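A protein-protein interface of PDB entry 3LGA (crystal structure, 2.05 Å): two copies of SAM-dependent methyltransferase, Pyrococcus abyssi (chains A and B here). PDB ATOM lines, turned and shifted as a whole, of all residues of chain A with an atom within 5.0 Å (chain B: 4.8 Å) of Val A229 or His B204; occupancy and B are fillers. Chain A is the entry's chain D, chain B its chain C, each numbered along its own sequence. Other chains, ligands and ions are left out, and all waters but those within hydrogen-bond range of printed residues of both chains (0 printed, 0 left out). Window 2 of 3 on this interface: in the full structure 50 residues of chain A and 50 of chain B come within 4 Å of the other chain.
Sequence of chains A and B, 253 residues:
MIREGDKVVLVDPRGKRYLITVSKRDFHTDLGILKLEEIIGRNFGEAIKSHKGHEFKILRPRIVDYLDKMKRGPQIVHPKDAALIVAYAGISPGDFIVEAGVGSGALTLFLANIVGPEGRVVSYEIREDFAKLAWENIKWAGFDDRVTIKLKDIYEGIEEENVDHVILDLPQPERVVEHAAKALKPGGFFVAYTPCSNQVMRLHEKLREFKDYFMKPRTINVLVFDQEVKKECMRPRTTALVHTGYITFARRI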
ATOM      1  N   GLN A 227      -0.769  10.279 -25.628  1.00  0.00           N
ATOM      2  CA  GLN A 227      -1.185   8.968 -25.135  1.00  0.00           C
ATOM      3  C   GLN A 227      -2.264   9.166 -24.088  1.00  0.00           C
ATOM      4  O   GLN A 227      -2.224  10.109 -23.305  1.00  0.00           O
ATOM      5  CB  GLN A 227      -0.022   8.166 -24.528  1.00  0.00           C
ATOM      6  CG  GLN A 227       1.164   8.008 -25.436  1.00  0.00           C
ATOM      7  CD  GLN A 227       0.836   7.174 -26.663  1.00  0.00           C
ATOM      8  OE1 GLN A 227       0.197   6.121 -26.556  1.00  0.00           O
ATOM      9  NE2 GLN A 227       1.223   7.677 -27.845  1.00  0.00           N
ATOM     10  N   GLU A 228      -3.243   8.277 -24.095  1.00  0.00           N
ATOM     11  CA  GLU A 228      -4.245   8.219 -23.055  1.00  0.00           C
ATOM     12  C   GLU A 228      -3.824   7.113 -22.105  1.00  0.00           C
ATOM     13  O   GLU A 228      -3.621   5.983 -22.517  1.00  0.00           O
ATOM     14  CB  GLU A 228      -5.608   7.910 -23.670  1.00  0.00           C
ATOM     15  CG  GLU A 228      -6.774   8.071 -22.701  1.00  0.00           C
ATOM     16  CD  GLU A 228      -8.051   7.396 -23.222  1.00  0.00           C
ATOM     17  OE1 GLU A 228      -8.838   8.113 -23.899  1.00  0.00           O
ATOM     18  OE2 GLU A 228      -8.249   6.162 -22.968  1.00  0.00           O
ATOM     19  N   VAL A 229      -3.634   7.444 -20.834  1.00  0.00           N
ATOM     20  CA  VAL A 229      -3.116   6.454 -19.891  1.00  0.00           C
ATOM     21  C   VAL A 229      -4.100   6.347 -18.734  1.00  0.00           C
ATOM     22  O   VAL A 229      -4.154   7.215 -17.861  1.00  0.00           O
ATOM     23  CB  VAL A 229      -1.675   6.756 -19.386  1.00  0.00           C
ATOM     24  CG1 VAL A 229      -1.109   5.547 -18.623  1.00  0.00           C
ATOM     25  CG2 VAL A 229      -0.727   7.174 -20.563  1.00  0.00           C
ATOM     26  N   LYS A 230      -4.922   5.312 -18.768  1.00  0.00           N
ATOM     27  CA  LYS A 230      -5.883   5.093 -17.685  1.00  0.00           C
ATOM     28  C   LYS A 230      -5.514   3.801 -16.985  1.00  0.00           C
ATOM     29  O   LYS A 230      -4.733   3.027 -17.516  1.00  0.00           O
ATOM     30  CB  LYS A 230      -7.310   5.091 -18.231  1.00  0.00           C
ATOM     31  CG  LYS A 230      -7.687   6.441 -18.782  1.00  0.00           C
ATOM     32  CD  LYS A 230      -9.089   6.475 -19.351  1.00  0.00           C
ATOM     33  CE  LYS A 230      -9.791   7.793 -18.977  1.00  0.00           C
ATOM     34  NZ  LYS A 230     -11.207   7.872 -19.485  1.00  0.00           N
ATOM     35  N   LYS A 231      -6.034   3.585 -15.776  1.00  0.00           N
ATOM     36  CA  LYS A 231      -5.649   2.420 -14.978  1.00  0.00           C
ATOM     37  C   LYS A 231      -5.722   1.134 -15.789  1.00  0.00           C
ATOM     38  O   LYS A 231      -4.812   0.293 -15.719  1.00  0.00           O
ATOM     39  CB  LYS A 231      -6.508   2.307 -13.706  1.00  0.00           C
ATOM     40  CG  LYS A 231      -6.126   1.119 -12.814  1.00  0.00           C
ATOM     41  CD  LYS A 231      -7.050   1.008 -11.597  1.00  0.00           C
ATOM     42  CE  LYS A 231      -6.641  -0.165 -10.697  1.00  0.00           C
ATOM     43  NZ  LYS A 231      -7.092   0.071  -9.259  1.00  0.00           N
ATOM     44  N   CYS A 233      -6.378   0.966 -19.320  1.00  0.00           N
ATOM     45  CA  CYS A 233      -6.154   1.110 -20.761  1.00  0.00           C
ATOM     46  C   CYS A 233      -5.165   2.231 -21.103  1.00  0.00           C
ATOM     47  O   CYS A 233      -5.402   3.417 -20.821  1.00  0.00           O
ATOM     48  CB  CYS A 233      -7.486   1.280 -21.523  1.00  0.00           C
ATOM     49  SG  CYS A 233      -7.361   1.439 -23.384  1.00  0.00           S
ATOM     50  N   MET A 234      -4.057   1.846 -21.721  1.00  0.00           N
ATOM     51  CA  MET A 234      -3.204   2.811 -22.386  1.00  0.00           C
ATOM     52  C   MET A 234      -3.291   2.631 -23.901  1.00  0.00           C
ATOM     53  O   MET A 234      -3.111   1.515 -24.418  1.00  0.00           O
ATOM     54  CB  MET A 234      -1.753   2.652 -21.943  1.00  0.00           C
ATOM     55  CG  MET A 234      -0.815   3.664 -22.672  1.00  0.00           C
ATOM     56  SD  MET A 234       0.860   3.432 -22.075  1.00  0.00           S
ATOM     57  CE  MET A 234       1.809   4.484 -23.224  1.00  0.00           C
ATOM     58  N   VAL B 200       5.489   3.649 -18.775  1.00  0.00           N
ATOM     59  CA  VAL B 200       4.487   4.728 -18.727  1.00  0.00           C
ATOM     60  C   VAL B 200       3.344   4.393 -17.741  1.00  0.00           C
ATOM     61  O   VAL B 200       2.906   5.245 -16.952  1.00  0.00           O
ATOM     62  CB  VAL B 200       3.917   5.057 -20.148  1.00  0.00           C
ATOM     63  CG1 VAL B 200       2.806   6.103 -20.078  1.00  0.00           C
ATOM     64  CG2 VAL B 200       5.054   5.518 -21.083  1.00  0.00           C
ATOM     65  N   MET B 201       2.849   3.151 -17.796  1.00  0.00           N
ATOM     66  CA  MET B 201       1.743   2.723 -16.917  1.00  0.00           C
ATOM     67  C   MET B 201       2.162   2.777 -15.439  1.00  0.00           C
ATOM     68  O   MET B 201       1.433   3.336 -14.597  1.00  0.00           O
ATOM     69  CB  MET B 201       1.308   1.286 -17.243  1.00  0.00           C
ATOM     70  CG  MET B 201       0.752   1.049 -18.648  1.00  0.00           C
ATOM     71  SD  MET B 201       0.644  -0.736 -19.018  1.00  0.00           S
ATOM     72  CE  MET B 201       0.231  -0.686 -20.774  1.00  0.00           C
ATOM     73  N   ARG B 202       3.323   2.212 -15.121  1.00  0.00           N
ATOM     74  CA  ARG B 202       3.848   2.280 -13.732  1.00  0.00           C
ATOM     75  C   ARG B 202       4.047   3.712 -13.267  1.00  0.00           C
ATOM     76  O   ARG B 202       3.673   4.081 -12.142  1.00  0.00           O
ATOM     77  CB  ARG B 202       5.156   1.532 -13.598  1.00  0.00           C
ATOM     78  CG  ARG B 202       5.007   0.033 -13.563  1.00  0.00           C
ATOM     79  CD  ARG B 202       6.378  -0.610 -13.309  1.00  0.00           C
ATOM     80  NE  ARG B 202       6.946  -1.181 -14.529  1.00  0.00           N
ATOM     81  CZ  ARG B 202       8.082  -0.794 -15.108  1.00  0.00           C
ATOM     82  NH1 ARG B 202       8.841   0.219 -14.580  1.00  0.00           N
ATOM     83  NH2 ARG B 202       8.470  -1.431 -16.224  1.00  0.00           N
ATOM     84  N   LEU B 203       4.585   4.553 -14.153  1.00  0.00           N
ATOM     85  CA  LEU B 203       4.753   5.959 -13.801  1.00  0.00           C
ATOM     86  C   LEU B 203       3.448   6.643 -13.556  1.00  0.00           C
ATOM     87  O   LEU B 203       3.313   7.422 -12.588  1.00  0.00           O
ATOM     88  CB  LEU B 203       5.559   6.727 -14.870  1.00  0.00           C
ATOM     89  CG  LEU B 203       5.775   8.222 -14.635  1.00  0.00           C
ATOM     90  CD1 LEU B 203       6.484   8.518 -13.237  1.00  0.00           C
ATOM     91  CD2 LEU B 203       6.621   8.772 -15.821  1.00  0.00           C
ATOM     92  N   HIS B 204       2.475   6.419 -14.435  1.00  0.00           N
ATOM     93  CA  HIS B 204       1.203   7.092 -14.230  1.00  0.00           C
ATOM     94  C   HIS B 204       0.484   6.652 -12.936  1.00  0.00           C
ATOM     95  O   HIS B 204      -0.199   7.461 -12.300  1.00  0.00           O
ATOM     96  CB  HIS B 204       0.281   6.913 -15.428  1.00  0.00           C
ATOM     97  CG  HIS B 204       0.468   7.955 -16.484  1.00  0.00           C
ATOM     98  ND1 HIS B 204      -0.435   8.970 -16.695  1.00  0.00           N
ATOM     99  CD2 HIS B 204       1.465   8.145 -17.383  1.00  0.00           C
ATOM    100  CE1 HIS B 204      -0.015   9.735 -17.688  1.00  0.00           C
ATOM    101  NE2 HIS B 204       1.131   9.252 -18.127  1.00  0.00           N
ATOM    102  N   GLU B 205       0.612   5.381 -12.578  1.00  0.00           N
ATOM    103  CA  GLU B 205       0.029   4.875 -11.314  1.00  0.00           C
ATOM    104  C   GLU B 205       0.635   5.617 -10.103  1.00  0.00           C
ATOM    105  O   GLU B 205      -0.082   6.086  -9.208  1.00  0.00           O
ATOM    106  CB  GLU B 205       0.264   3.367 -11.242  1.00  0.00           C
ATOM    107  CG  GLU B 205      -0.061   2.728  -9.919  1.00  0.00           C
ATOM    108  CD  GLU B 205       0.030   1.231 -10.015  1.00  0.00           C
ATOM    109  OE1 GLU B 205       0.742   0.610  -9.192  1.00  0.00           O
ATOM    110  OE2 GLU B 205      -0.591   0.671 -10.953  1.00  0.00           O
ATOM    111  N   LYS B 206       1.958   5.803 -10.130  1.00  0.00           N
ATOM    112  CA  LYS B 206       2.627   6.611  -9.115  1.00  0.00           C
ATOM    113  C   LYS B 206       2.155   8.059  -9.113  1.00  0.00           C
ATOM    114  O   LYS B 206       1.868   8.625  -8.051  1.00  0.00           O
ATOM    115  CB  LYS B 206       4.150   6.517  -9.232  1.00  0.00           C
ATOM    116  CG  LYS B 206       4.921   7.248  -8.097  1.00  0.00           C
ATOM    117  CD  LYS B 206       4.623   6.690  -6.687  1.00  0.00           C
ATOM    118  CE  LYS B 206       5.194   5.300  -6.539  1.00  0.00           C
ATOM    119  NZ  LYS B 206       5.202   4.903  -5.092  1.00  0.00           N
ATOM    120  N   LEU B 207       2.072   8.672 -10.292  1.00  0.00           N
ATOM    121  CA  LEU B 207       1.579  10.047 -10.358  1.00  0.00           C
ATOM    122  C   LEU B 207       0.131  10.163  -9.868  1.00  0.00           C
ATOM    123  O   LEU B 207      -0.222  11.173  -9.310  1.00  0.00           O
ATOM    124  CB  LEU B 207       1.758  10.661 -11.771  1.00  0.00           C
ATOM    125  CG  LEU B 207       3.233  10.874 -12.200  1.00  0.00           C
ATOM    126  CD1 LEU B 207       3.405  11.017 -13.732  1.00  0.00           C
ATOM    127  CD2 LEU B 207       3.819  12.073 -11.449  1.00  0.00           C
ATOM    128  N   ARG B 208      -0.696   9.147 -10.092  1.00  0.00           N
ATOM    129  CA  ARG B 208      -2.086   9.137  -9.549  1.00  0.00           C
ATOM    130  C   ARG B 208      -2.038   9.109  -8.002  1.00  0.00           C
ATOM    131  O   ARG B 208      -2.742   9.862  -7.343  1.00  0.00           O
ATOM    132  CB  ARG B 208      -2.904   7.934 -10.064  1.00  0.00           C
ATOM    133  CG  ARG B 208      -3.260   7.945 -11.570  1.00  0.00           C
ATOM    134  CD  ARG B 208      -4.401   6.916 -11.980  1.00  0.00           C
ATOM    135  NE  ARG B 208      -3.987   5.511 -11.846  1.00  0.00           N
ATOM    136  CZ  ARG B 208      -3.347   4.818 -12.793  1.00  0.00           C
ATOM    137  NH1 ARG B 208      -3.052   5.385 -13.979  1.00  0.00           N
ATOM    138  NH2 ARG B 208      -2.994   3.556 -12.540  1.00  0.00           N
ATOM    139  N   PRO B 217      -0.994  14.660 -15.532  1.00  0.00           N
ATOM    140  CA  PRO B 217       0.201  14.335 -16.344  1.00  0.00           C
ATOM    141  C   PRO B 217      -0.170  14.204 -17.822  1.00  0.00           C
ATOM    142  O   PRO B 217      -1.339  13.926 -18.140  1.00  0.00           O
ATOM    143  CB  PRO B 217       0.683  12.977 -15.805  1.00  0.00           C
ATOM    144  CG  PRO B 217      -0.315  12.570 -14.729  1.00  0.00           C
ATOM    145  CD  PRO B 217      -1.468  13.516 -14.730  1.00  0.00           C
ATOM    146  N   THR B 219       1.459  12.434 -21.553  1.00  0.00           N
ATOM    147  CA  THR B 219       2.489  11.582 -22.147  1.00  0.00           C
ATOM    148  C   THR B 219       2.376  11.712 -23.640  1.00  0.00           C
ATOM    149  O   THR B 219       1.257  11.658 -24.199  1.00  0.00           O
ATOM    150  CB  THR B 219       2.333  10.086 -21.721  1.00  0.00           C
ATOM    151  OG1 THR B 219       2.540   9.985 -20.318  1.00  0.00           O
ATOM    152  CG2 THR B 219       3.336   9.200 -22.407  1.00  0.00           C
ATOM    153  N   THR B 248       6.751  11.837 -20.496  1.00  0.00           N
ATOM    154  CA  THR B 248       5.688  12.237 -19.580  1.00  0.00           C
ATOM    155  C   THR B 248       6.035  13.497 -18.787  1.00  0.00           C
ATOM    156  O   THR B 248       7.154  13.594 -18.268  1.00  0.00           O
ATOM    157  CB  THR B 248       5.374  11.066 -18.556  1.00  0.00           C
ATOM    158  OG1 THR B 248       4.986   9.909 -19.286  1.00  0.00           O
ATOM    159  CG2 THR B 248       4.246  11.457 -17.536  1.00  0.00           C
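The backbone carbonyl oxygen of Thr B219 sits at hydrogen-bond distance from the backbone NH of Gln A227.
A ring nitrogen (NE2) of His B204 lies within hydrogen-bond range of the side-chain hydroxyl (OG1) of Thr B219 (2.7 Å).
The side-chain hydroxyl (OG1) of Thr B219 sits at hydrogen-bond distance from the side-chain hydroxyl (OG1) of Thr B248, at 2.7 Å.
Among the printed residues, merely in contact across the chains: Val A229 with His B204, Met A234 with Val B200, Val A229 with Val B200 and Lys A231 with Arg B208.
Printed residues of chain B within 4 Å of Gln A227: Thr B219 (2.8 Å).
Of the printed residues of chain B, Val A229 touches Val B200 (3.7 Å) and His B204 (3.6 Å).
Cys A233 touches none of the printed residues of chain B.
His B204 touches one residue of chain A.
Of the printed residues of chain A, Arg B208 touches Lys A231.
Thr B248 touches none of the printed residues of chain A.
The nearest printed residue of chain A that does not touch His B204 is Gln A227 (6.0 Å).
The nearest printed residue of chain A that does not touch Arg B208 is Lys A230 (4.2 Å).
Of the 7 printed residues of chain A, 4 touch a printed residue of chain B.
Printed residues of chain A that touch a printed residue of chain B: Gln A227, Val A229, Lys A231 and Met A234.
Hydrophobic or aromatic side chains of chain A within 4 Å of the printed part of chain B: Val A229 and Met A234.
No position is printed for both chains.
Of the 5 pairs that touch across the chains among the printed residues, none has its exchanged pair printed and touching as well.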
